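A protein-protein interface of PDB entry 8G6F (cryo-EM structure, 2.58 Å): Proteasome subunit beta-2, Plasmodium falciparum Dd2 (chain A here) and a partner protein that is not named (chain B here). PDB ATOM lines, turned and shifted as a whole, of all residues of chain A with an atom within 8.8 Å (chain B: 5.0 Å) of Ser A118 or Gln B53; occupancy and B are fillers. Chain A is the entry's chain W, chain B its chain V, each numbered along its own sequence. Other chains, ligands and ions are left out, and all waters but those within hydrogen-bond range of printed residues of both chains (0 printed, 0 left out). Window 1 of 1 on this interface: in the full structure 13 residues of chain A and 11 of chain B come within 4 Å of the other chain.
The backbone NH (N) of Ser A119 lies within hydrogen-bond range of the side-chain amide oxygen (OE1) of Gln B53, at 3.0 Å. The side-chain amino group (NZ) of Lys B54 lies within hydrogen-bond range of the side-chain hydroxyl (OG1) of Thr A84 (3.4 Å). OE2 of Glu B57 lies within hydrogen-bond range of NE2 of Gln A85.
OG of Ser B52 is in hydrogen-bond range of O of Ser B49 (3.2 Å). NZ of Lys B54 lies within salt-bridge range of OE1 of Glu B57, 3.0 Å away. The side-chain hydroxyl of Thr A84 is in hydrogen-bond range of the backbone carbonyl oxygen of Val A80 (2.4 Å).
His B51 touches Phe A88. CG of Lys B54 touches CD1 of Phe A88 (3.5 Å). His A116 touches Ala B50. Ala B50 touches Gly A117. O of Gly A117 touches CE of Lys B54 (3.4 Å). Ser A118 touches Ser B49 (CB to CB, 3.9 Å). Ser A118 touches Ala B50 (CB to N, 3.8 Å). Gln B53 touches Ser A118.
Printed residues of chain B within 4 Å of Gln A85: Glu B57. Of the printed residues of chain B, Phe A88 touches His B51 (3.98 Å) and Lys B54 (3.5 Å). Ile A113 touches none of the printed residues of chain B. Pro A115 touches none of the printed residues of chain B. Ser A118 touches three residues of chain B. Of the printed residues of chain B, Ser A119 touches Gln B53. Printed residues of chain A within 4 Å of Ser B49: Ser A118. Of chain A, only His A116, Gly A117 and Ser A118 come within 4 Å of Ala B50. Of the printed residues of chain A, His B51 touches Phe A88. Of chain A, only Thr A84 (3.4 Å), Phe A88 (3.5 Å) and Gly A117 (3.4 Å) come within 4 Å of Lys B54. The nearest residue of chain A that does not touch Gln B53 is Gly A117 (4.3 Å). The nearest printed residue of chain A that does not touch His B51 is His A116 (5.7 Å).
Hydrophobic or aromatic side chains of chain B within 4 Å of the printed part of chain A: Ala B50 and His B51. Printed residues of chain A that touch a printed residue of chain B: Thr A84, Gln A85, Phe A88, His A116, Gly A117, Ser A118 and Ser A119. Hydrophobic or aromatic side chains of chain A within 4 Å of the printed part of chain B: Phe A88. Among the printed residues, 11 pairs touch across the chains. Among the printed residues, no Asp or Glu carboxylate lies within 4 Å of a Lys or Arg side-chain nitrogen of the other chain.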
ATOM      1  N   VAL A  80     -20.018   9.510  27.150  1.00  0.00           N
ATOM      2  CA  VAL A  80     -19.903   8.541  26.065  1.00  0.00           C
ATOM      3  C   VAL A  80     -20.236   7.144  26.571  1.00  0.00           C
ATOM      4  O   VAL A  80     -20.999   6.404  25.943  1.00  0.00           O
ATOM      5  CB  VAL A  80     -18.497   8.599  25.443  1.00  0.00           C
ATOM      6  CG1 VAL A  80     -18.248   7.387  24.568  1.00  0.00           C
ATOM      7  CG2 VAL A  80     -18.333   9.865  24.645  1.00  0.00           C
ATOM      8  N   LEU A  83     -24.066   6.803  27.473  1.00  0.00           N
ATOM      9  CA  LEU A  83     -24.904   6.831  26.282  1.00  0.00           C
ATOM     10  C   LEU A  83     -24.746   5.559  25.466  1.00  0.00           C
ATOM     11  O   LEU A  83     -25.737   4.966  25.027  1.00  0.00           O
ATOM     12  CB  LEU A  83     -24.550   8.055  25.440  1.00  0.00           C
ATOM     13  CG  LEU A  83     -25.686   8.848  24.806  1.00  0.00           C
ATOM     14  CD1 LEU A  83     -26.728   9.244  25.837  1.00  0.00           C
ATOM     15  CD2 LEU A  83     -25.115  10.071  24.124  1.00  0.00           C
ATOM     16  N   THR A  84     -23.505   5.131  25.233  1.00  0.00           N
ATOM     17  CA  THR A  84     -23.292   3.942  24.419  1.00  0.00           C
ATOM     18  C   THR A  84     -23.862   2.708  25.094  1.00  0.00           C
ATOM     19  O   THR A  84     -24.445   1.851  24.427  1.00  0.00           O
ATOM     20  CB  THR A  84     -21.807   3.747  24.130  1.00  0.00           C
ATOM     21  OG1 THR A  84     -21.037   4.094  25.283  1.00  0.00           O
ATOM     22  CG2 THR A  84     -21.379   4.603  22.964  1.00  0.00           C
ATOM     23  N   GLN A  85     -23.700   2.588  26.413  1.00  0.00           N
ATOM     24  CA  GLN A  85     -24.245   1.425  27.099  1.00  0.00           C
ATOM     25  C   GLN A  85     -25.764   1.393  27.000  1.00  0.00           C
ATOM     26  O   GLN A  85     -26.350   0.339  26.739  1.00  0.00           O
ATOM     27  CB  GLN A  85     -23.784   1.417  28.553  1.00  0.00           C
ATOM     28  CG  GLN A  85     -22.357   0.925  28.716  1.00  0.00           C
ATOM     29  CD  GLN A  85     -21.738   1.332  30.032  1.00  0.00           C
ATOM     30  OE1 GLN A  85     -22.416   1.844  30.918  1.00  0.00           O
ATOM     31  NE2 GLN A  85     -20.441   1.106  30.169  1.00  0.00           N
ATOM     32  N   LEU A  87     -27.675   2.822  24.602  1.00  0.00           N
ATOM     33  CA  LEU A  87     -28.070   2.570  23.222  1.00  0.00           C
ATOM     34  C   LEU A  87     -27.840   1.114  22.845  1.00  0.00           C
ATOM     35  O   LEU A  87     -28.660   0.510  22.146  1.00  0.00           O
ATOM     36  CB  LEU A  87     -27.303   3.501  22.284  1.00  0.00           C
ATOM     37  CG  LEU A  87     -27.632   4.989  22.403  1.00  0.00           C
ATOM     38  CD1 LEU A  87     -26.632   5.815  21.636  1.00  0.00           C
ATOM     39  CD2 LEU A  87     -29.034   5.281  21.920  1.00  0.00           C
ATOM     40  N   PHE A  88     -26.724   0.536  23.291  1.00  0.00           N
ATOM     41  CA  PHE A  88     -26.469  -0.875  23.042  1.00  0.00           C
ATOM     42  C   PHE A  88     -27.510  -1.746  23.722  1.00  0.00           C
ATOM     43  O   PHE A  88     -27.996  -2.718  23.134  1.00  0.00           O
ATOM     44  CB  PHE A  88     -25.069  -1.241  23.524  1.00  0.00           C
ATOM     45  CG  PHE A  88     -24.702  -2.674  23.286  1.00  0.00           C
ATOM     46  CD1 PHE A  88     -24.288  -3.098  22.038  1.00  0.00           C
ATOM     47  CD2 PHE A  88     -24.768  -3.594  24.310  1.00  0.00           C
ATOM     48  CE1 PHE A  88     -23.946  -4.406  21.822  1.00  0.00           C
ATOM     49  CE2 PHE A  88     -24.433  -4.904  24.093  1.00  0.00           C
ATOM     50  CZ  PHE A  88     -24.019  -5.311  22.850  1.00  0.00           C
ATOM     51  N   GLY A  92     -30.282  -0.360  19.147  1.00  0.00           N
ATOM     52  CA  GLY A  92     -30.591   0.500  18.030  1.00  0.00           C
ATOM     53  C   GLY A  92     -32.048   0.864  17.886  1.00  0.00           C
ATOM     54  O   GLY A  92     -32.403   1.542  16.915  1.00  0.00           O
ATOM     55  N   CYS A  96     -30.951   7.275  17.984  1.00  0.00           N
ATOM     56  CA  CYS A  96     -30.283   8.483  18.454  1.00  0.00           C
ATOM     57  C   CYS A  96     -28.858   8.493  17.923  1.00  0.00           C
ATOM     58  O   CYS A  96     -28.007   7.752  18.422  1.00  0.00           O
ATOM     59  CB  CYS A  96     -30.275   8.551  19.980  1.00  0.00           C
ATOM     60  SG  CYS A  96     -31.880   8.476  20.758  1.00  0.00           S
ATOM     61  N   ALA A  97     -28.594   9.326  16.924  1.00  0.00           N
ATOM     62  CA  ALA A  97     -27.238   9.611  16.481  1.00  0.00           C
ATOM     63  C   ALA A  97     -26.835  10.952  17.077  1.00  0.00           C
ATOM     64  O   ALA A  97     -27.471  11.970  16.800  1.00  0.00           O
ATOM     65  CB  ALA A  97     -27.151   9.635  14.957  1.00  0.00           C
ATOM     66  N   ILE A  98     -25.788  10.952  17.893  1.00  0.00           N
ATOM     67  CA  ILE A  98     -25.435  12.101  18.716  1.00  0.00           C
ATOM     68  C   ILE A  98     -24.023  12.555  18.376  1.00  0.00           C
ATOM     69  O   ILE A  98     -23.108  11.735  18.263  1.00  0.00           O
ATOM     70  CB  ILE A  98     -25.557  11.772  20.215  1.00  0.00           C
ATOM     71  CG1 ILE A  98     -27.027  11.612  20.600  1.00  0.00           C
ATOM     72  CG2 ILE A  98     -24.917  12.859  21.057  1.00  0.00           C
ATOM     73  CD1 ILE A  98     -27.390  10.220  21.025  1.00  0.00           C
ATOM     74  N   TYR A 111     -17.192  13.433  19.889  1.00  0.00           N
ATOM     75  CA  TYR A 111     -17.561  12.045  19.690  1.00  0.00           C
ATOM     76  C   TYR A 111     -18.769  11.963  18.779  1.00  0.00           C
ATOM     77  O   TYR A 111     -19.685  12.781  18.874  1.00  0.00           O
ATOM     78  CB  TYR A 111     -17.895  11.358  21.008  1.00  0.00           C
ATOM     79  CG  TYR A 111     -16.713  11.131  21.900  1.00  0.00           C
ATOM     80  CD1 TYR A 111     -16.331  12.085  22.823  1.00  0.00           C
ATOM     81  CD2 TYR A 111     -15.982   9.958  21.828  1.00  0.00           C
ATOM     82  CE1 TYR A 111     -15.256  11.885  23.643  1.00  0.00           C
ATOM     83  CE2 TYR A 111     -14.904   9.749  22.647  1.00  0.00           C
ATOM     84  CZ  TYR A 111     -14.548  10.716  23.554  1.00  0.00           C
ATOM     85  OH  TYR A 111     -13.470  10.520  24.380  1.00  0.00           O
ATOM     86  N   GLY A 112     -18.755  10.969  17.896  1.00  0.00           N
ATOM     87  CA  GLY A 112     -19.945  10.551  17.185  1.00  0.00           C
ATOM     88  C   GLY A 112     -20.436   9.246  17.780  1.00  0.00           C
ATOM     89  O   GLY A 112     -19.670   8.296  17.927  1.00  0.00           O
ATOM     90  N   ILE A 113     -21.716   9.222  18.140  1.00  0.00           N
ATOM     91  CA  ILE A 113     -22.361   8.062  18.740  1.00  0.00           C
ATOM     92  C   ILE A 113     -23.521   7.670  17.844  1.00  0.00           C
ATOM     93  O   ILE A 113     -24.291   8.532  17.412  1.00  0.00           O
ATOM     94  CB  ILE A 113     -22.848   8.353  20.171  1.00  0.00           C
ATOM     95  CG1 ILE A 113     -21.664   8.643  21.091  1.00  0.00           C
ATOM     96  CG2 ILE A 113     -23.651   7.187  20.709  1.00  0.00           C
ATOM     97  CD1 ILE A 113     -21.474  10.092  21.384  1.00  0.00           C
ATOM     98  N   HIS A 114     -23.646   6.384  17.567  1.00  0.00           N
ATOM     99  CA  HIS A 114     -24.649   5.877  16.654  1.00  0.00           C
ATOM    100  C   HIS A 114     -25.683   5.039  17.392  1.00  0.00           C
ATOM    101  O   HIS A 114     -25.429   4.545  18.493  1.00  0.00           O
ATOM    102  CB  HIS A 114     -23.976   5.057  15.551  1.00  0.00           C
ATOM    103  CG  HIS A 114     -22.937   5.826  14.798  1.00  0.00           C
ATOM    104  ND1 HIS A 114     -21.627   5.914  15.218  1.00  0.00           N
ATOM    105  CD2 HIS A 114     -23.023   6.574  13.674  1.00  0.00           C
ATOM    106  CE1 HIS A 114     -20.947   6.669  14.374  1.00  0.00           C
ATOM    107  NE2 HIS A 114     -21.770   7.080  13.427  1.00  0.00           N
ATOM    108  N   PRO A 115     -26.872   4.863  16.810  1.00  0.00           N
ATOM    109  CA  PRO A 115     -27.989   4.300  17.585  1.00  0.00           C
ATOM    110  C   PRO A 115     -27.715   2.930  18.173  1.00  0.00           C
ATOM    111  O   PRO A 115     -28.302   2.590  19.204  1.00  0.00           O
ATOM    112  CB  PRO A 115     -29.129   4.251  16.560  1.00  0.00           C
ATOM    113  CG  PRO A 115     -28.761   5.226  15.525  1.00  0.00           C
ATOM    114  CD  PRO A 115     -27.277   5.218  15.444  1.00  0.00           C
ATOM    115  N   HIS A 116     -26.861   2.124  17.549  1.00  0.00           N
ATOM    116  CA  HIS A 116     -26.599   0.782  18.044  1.00  0.00           C
ATOM    117  C   HIS A 116     -25.607   0.756  19.197  1.00  0.00           C
ATOM    118  O   HIS A 116     -25.417  -0.303  19.800  1.00  0.00           O
ATOM    119  CB  HIS A 116     -26.082  -0.101  16.912  1.00  0.00           C
ATOM    120  CG  HIS A 116     -27.150  -0.542  15.964  1.00  0.00           C
ATOM    121  ND1 HIS A 116     -27.531   0.210  14.875  1.00  0.00           N
ATOM    122  CD2 HIS A 116     -27.924  -1.651  15.945  1.00  0.00           C
ATOM    123  CE1 HIS A 116     -28.491  -0.419  14.224  1.00  0.00           C
ATOM    124  NE2 HIS A 116     -28.747  -1.551  14.853  1.00  0.00           N
ATOM    125  N   GLY A 117     -24.982   1.876  19.517  1.00  0.00           N
ATOM    126  CA  GLY A 117     -24.082   1.968  20.635  1.00  0.00           C
ATOM    127  C   GLY A 117     -22.607   2.001  20.304  1.00  0.00           C
ATOM    128  O   GLY A 117     -21.794   1.712  21.188  1.00  0.00           O
ATOM    129  N   SER A 118     -22.233   2.319  19.072  1.00  0.00           N
ATOM    130  CA  SER A 118     -20.836   2.543  18.741  1.00  0.00           C
ATOM    131  C   SER A 118     -20.506   4.019  18.905  1.00  0.00           C
ATOM    132  O   SER A 118     -21.375   4.886  18.799  1.00  0.00           O
ATOM    133  CB  SER A 118     -20.522   2.093  17.314  1.00  0.00           C
ATOM    134  OG  SER A 118     -21.619   2.301  16.451  1.00  0.00           O
ATOM    135  N   SER A 119     -19.238   4.296  19.183  1.00  0.00           N
ATOM    136  CA  SER A 119     -18.769   5.661  19.334  1.00  0.00           C
ATOM    137  C   SER A 119     -17.409   5.795  18.668  1.00  0.00           C
ATOM    138  O   SER A 119     -16.688   4.816  18.475  1.00  0.00           O
ATOM    139  CB  SER A 119     -18.680   6.072  20.805  1.00  0.00           C
ATOM    140  OG  SER A 119     -17.357   5.949  21.289  1.00  0.00           O
ATOM    141  N   CYS A 120     -17.077   7.027  18.301  1.00  0.00           N
ATOM    142  CA  CYS A 120     -15.774   7.320  17.727  1.00  0.00           C
ATOM    143  C   CYS A 120     -15.363   8.734  18.103  1.00  0.00           C
ATOM    144  O   CYS A 120     -16.173   9.658  18.042  1.00  0.00           O
ATOM    145  CB  CYS A 120     -15.782   7.167  16.205  1.00  0.00           C
ATOM    146  SG  CYS A 120     -14.138   7.034  15.472  1.00  0.00           S
ATOM    147  N   LEU A 121     -14.098   8.888  18.481  1.00  0.00           N
ATOM    148  CA  LEU A 121     -13.518  10.189  18.781  1.00  0.00           C
ATOM    149  C   LEU A 121     -12.982  10.795  17.491  1.00  0.00           C
ATOM    150  O   LEU A 121     -12.132  10.197  16.828  1.00  0.00           O
ATOM    151  CB  LEU A 121     -12.412  10.044  19.822  1.00  0.00           C
ATOM    152  CG  LEU A 121     -11.651  11.302  20.233  1.00  0.00           C
ATOM    153  CD1 LEU A 121     -12.425  12.086  21.265  1.00  0.00           C
ATOM    154  CD2 LEU A 121     -10.286  10.924  20.766  1.00  0.00           C
ATOM    155  N   LEU A 127     -23.885  14.462  11.299  1.00  0.00           N
ATOM    156  CA  LEU A 127     -24.919  13.438  11.329  1.00  0.00           C
ATOM    157  C   LEU A 127     -26.242  14.040  10.877  1.00  0.00           C
ATOM    158  O   LEU A 127     -26.411  15.262  10.805  1.00  0.00           O
ATOM    159  CB  LEU A 127     -25.064  12.819  12.724  1.00  0.00           C
ATOM    160  CG  LEU A 127     -23.859  12.035  13.250  1.00  0.00           C
ATOM    161  CD1 LEU A 127     -24.012  11.754  14.725  1.00  0.00           C
ATOM    162  CD2 LEU A 127     -23.670  10.740  12.486  1.00  0.00           C
ATOM    163  N   ARG B  45     -10.226  -5.760  16.507  1.00  0.00           N
ATOM    164  CA  ARG B  45     -11.664  -5.954  16.402  1.00  0.00           C
ATOM    165  C   ARG B  45     -12.099  -6.006  14.945  1.00  0.00           C
ATOM    166  O   ARG B  45     -11.577  -5.270  14.105  1.00  0.00           O
ATOM    167  CB  ARG B  45     -12.423  -4.827  17.104  1.00  0.00           C
ATOM    168  CG  ARG B  45     -11.810  -4.350  18.398  1.00  0.00           C
ATOM    169  CD  ARG B  45     -12.680  -3.297  19.059  1.00  0.00           C
ATOM    170  NE  ARG B  45     -12.373  -1.949  18.595  1.00  0.00           N
ATOM    171  CZ  ARG B  45     -13.120  -1.239  17.759  1.00  0.00           C
ATOM    172  NH1 ARG B  45     -14.241  -1.721  17.248  1.00  0.00           N
ATOM    173  NH2 ARG B  45     -12.734  -0.012  17.430  1.00  0.00           N
ATOM    174  N   ALA B  48     -19.239  -5.996  13.681  1.00  0.00           N
ATOM    175  CA  ALA B  48     -20.045  -4.847  14.068  1.00  0.00           C
ATOM    176  C   ALA B  48     -19.303  -3.999  15.095  1.00  0.00           C
ATOM    177  O   ALA B  48     -18.823  -4.509  16.114  1.00  0.00           O
ATOM    178  CB  ALA B  48     -21.388  -5.307  14.630  1.00  0.00           C
ATOM    179  N   SER B  49     -19.223  -2.695  14.825  1.00  0.00           N
ATOM    180  CA  SER B  49     -18.481  -1.802  15.705  1.00  0.00           C
ATOM    181  C   SER B  49     -19.092  -1.759  17.097  1.00  0.00           C
ATOM    182  O   SER B  49     -18.370  -1.806  18.096  1.00  0.00           O
ATOM    183  CB  SER B  49     -18.432  -0.399  15.106  1.00  0.00           C
ATOM    184  OG  SER B  49     -17.526  -0.344  14.023  1.00  0.00           O
ATOM    185  N   ALA B  50     -20.418  -1.675  17.186  1.00  0.00           N
ATOM    186  CA  ALA B  50     -21.063  -1.624  18.493  1.00  0.00           C
ATOM    187  C   ALA B  50     -20.773  -2.885  19.291  1.00  0.00           C
ATOM    188  O   ALA B  50     -20.397  -2.822  20.469  1.00  0.00           O
ATOM    189  CB  ALA B  50     -22.568  -1.433  18.321  1.00  0.00           C
ATOM    190  N   HIS B  51     -20.924  -4.046  18.654  1.00  0.00           N
ATOM    191  CA  HIS B  51     -20.701  -5.308  19.345  1.00  0.00           C
ATOM    192  C   HIS B  51     -19.268  -5.410  19.837  1.00  0.00           C
ATOM    193  O   HIS B  51     -19.020  -5.682  21.017  1.00  0.00           O
ATOM    194  CB  HIS B  51     -21.034  -6.475  18.416  1.00  0.00           C
ATOM    195  CG  HIS B  51     -22.443  -6.468  17.915  1.00  0.00           C
ATOM    196  ND1 HIS B  51     -22.972  -7.503  17.177  1.00  0.00           N
ATOM    197  CD2 HIS B  51     -23.433  -5.554  18.042  1.00  0.00           C
ATOM    198  CE1 HIS B  51     -24.227  -7.229  16.874  1.00  0.00           C
ATOM    199  NE2 HIS B  51     -24.531  -6.050  17.386  1.00  0.00           N
ATOM    200  N   SER B  52     -18.303  -5.181  18.945  1.00  0.00           N
ATOM    201  CA  SER B  52     -16.911  -5.336  19.342  1.00  0.00           C
ATOM    202  C   SER B  52     -16.522  -4.316  20.405  1.00  0.00           C
ATOM    203  O   SER B  52     -15.823  -4.657  21.361  1.00  0.00           O
ATOM    204  CB  SER B  52     -15.995  -5.234  18.125  1.00  0.00           C
ATOM    205  OG  SER B  52     -16.367  -4.174  17.272  1.00  0.00           O
ATOM    206  N   GLN B  53     -16.977  -3.068  20.277  1.00  0.00           N
ATOM    207  CA  GLN B  53     -16.608  -2.043  21.246  1.00  0.00           C
ATOM    208  C   GLN B  53     -17.175  -2.349  22.627  1.00  0.00           C
ATOM    209  O   GLN B  53     -16.470  -2.234  23.636  1.00  0.00           O
ATOM    210  CB  GLN B  53     -17.093  -0.678  20.763  1.00  0.00           C
ATOM    211  CG  GLN B  53     -16.227  -0.065  19.687  1.00  0.00           C
ATOM    212  CD  GLN B  53     -16.847   1.171  19.087  1.00  0.00           C
ATOM    213  OE1 GLN B  53     -17.733   1.778  19.677  1.00  0.00           O
ATOM    214  NE2 GLN B  53     -16.381   1.553  17.910  1.00  0.00           N
ATOM    215  N   LYS B  54     -18.450  -2.734  22.700  1.00  0.00           N
ATOM    216  CA  LYS B  54     -19.036  -3.019  24.004  1.00  0.00           C
ATOM    217  C   LYS B  54     -18.415  -4.261  24.628  1.00  0.00           C
ATOM    218  O   LYS B  54     -18.160  -4.298  25.843  1.00  0.00           O
ATOM    219  CB  LYS B  54     -20.548  -3.168  23.873  1.00  0.00           C
ATOM    220  CG  LYS B  54     -21.238  -1.904  23.394  1.00  0.00           C
ATOM    221  CD  LYS B  54     -21.050  -0.747  24.354  1.00  0.00           C
ATOM    222  CE  LYS B  54     -20.105   0.291  23.786  1.00  0.00           C
ATOM    223  NZ  LYS B  54     -19.453   1.096  24.848  1.00  0.00           N
ATOM    224  N   ILE B  55     -18.136  -5.279  23.813  1.00  0.00           N
ATOM    225  CA  ILE B  55     -17.458  -6.461  24.330  1.00  0.00           C
ATOM    226  C   ILE B  55     -16.095  -6.082  24.888  1.00  0.00           C
ATOM    227  O   ILE B  55     -15.710  -6.520  25.975  1.00  0.00           O
ATOM    228  CB  ILE B  55     -17.342  -7.536  23.234  1.00  0.00           C
ATOM    229  CG1 ILE B  55     -18.699  -8.191  22.975  1.00  0.00           C
ATOM    230  CG2 ILE B  55     -16.310  -8.583  23.619  1.00  0.00           C
ATOM    231  CD1 ILE B  55     -19.369  -8.743  24.211  1.00  0.00           C
ATOM    232  N   ILE B  56     -15.346  -5.260  24.155  1.00  0.00           N
ATOM    233  CA  ILE B  56     -14.002  -4.905  24.592  1.00  0.00           C
ATOM    234  C   ILE B  56     -14.054  -4.079  25.869  1.00  0.00           C
ATOM    235  O   ILE B  56     -13.184  -4.207  26.734  1.00  0.00           O
ATOM    236  CB  ILE B  56     -13.251  -4.174  23.462  1.00  0.00           C
ATOM    237  CG1 ILE B  56     -12.911  -5.138  22.320  1.00  0.00           C
ATOM    238  CG2 ILE B  56     -11.987  -3.526  23.986  1.00  0.00           C
ATOM    239  CD1 ILE B  56     -12.375  -6.487  22.753  1.00  0.00           C
ATOM    240  N   GLU B  57     -15.065  -3.226  26.018  1.00  0.00           N
ATOM    241  CA  GLU B  57     -15.207  -2.484  27.267  1.00  0.00           C
ATOM    242  C   GLU B  57     -15.442  -3.430  28.443  1.00  0.00           C
ATOM    243  O   GLU B  57     -14.795  -3.315  29.497  1.00  0.00           O
ATOM    244  CB  GLU B  57     -16.347  -1.477  27.144  1.00  0.00           C
ATOM    245  CG  GLU B  57     -16.430  -0.514  28.307  1.00  0.00           C
ATOM    246  CD  GLU B  57     -17.587   0.451  28.184  1.00  0.00           C
ATOM    247  OE1 GLU B  57     -18.570   0.118  27.491  1.00  0.00           O
ATOM    248  OE2 GLU B  57     -17.513   1.543  28.784  1.00  0.00           O
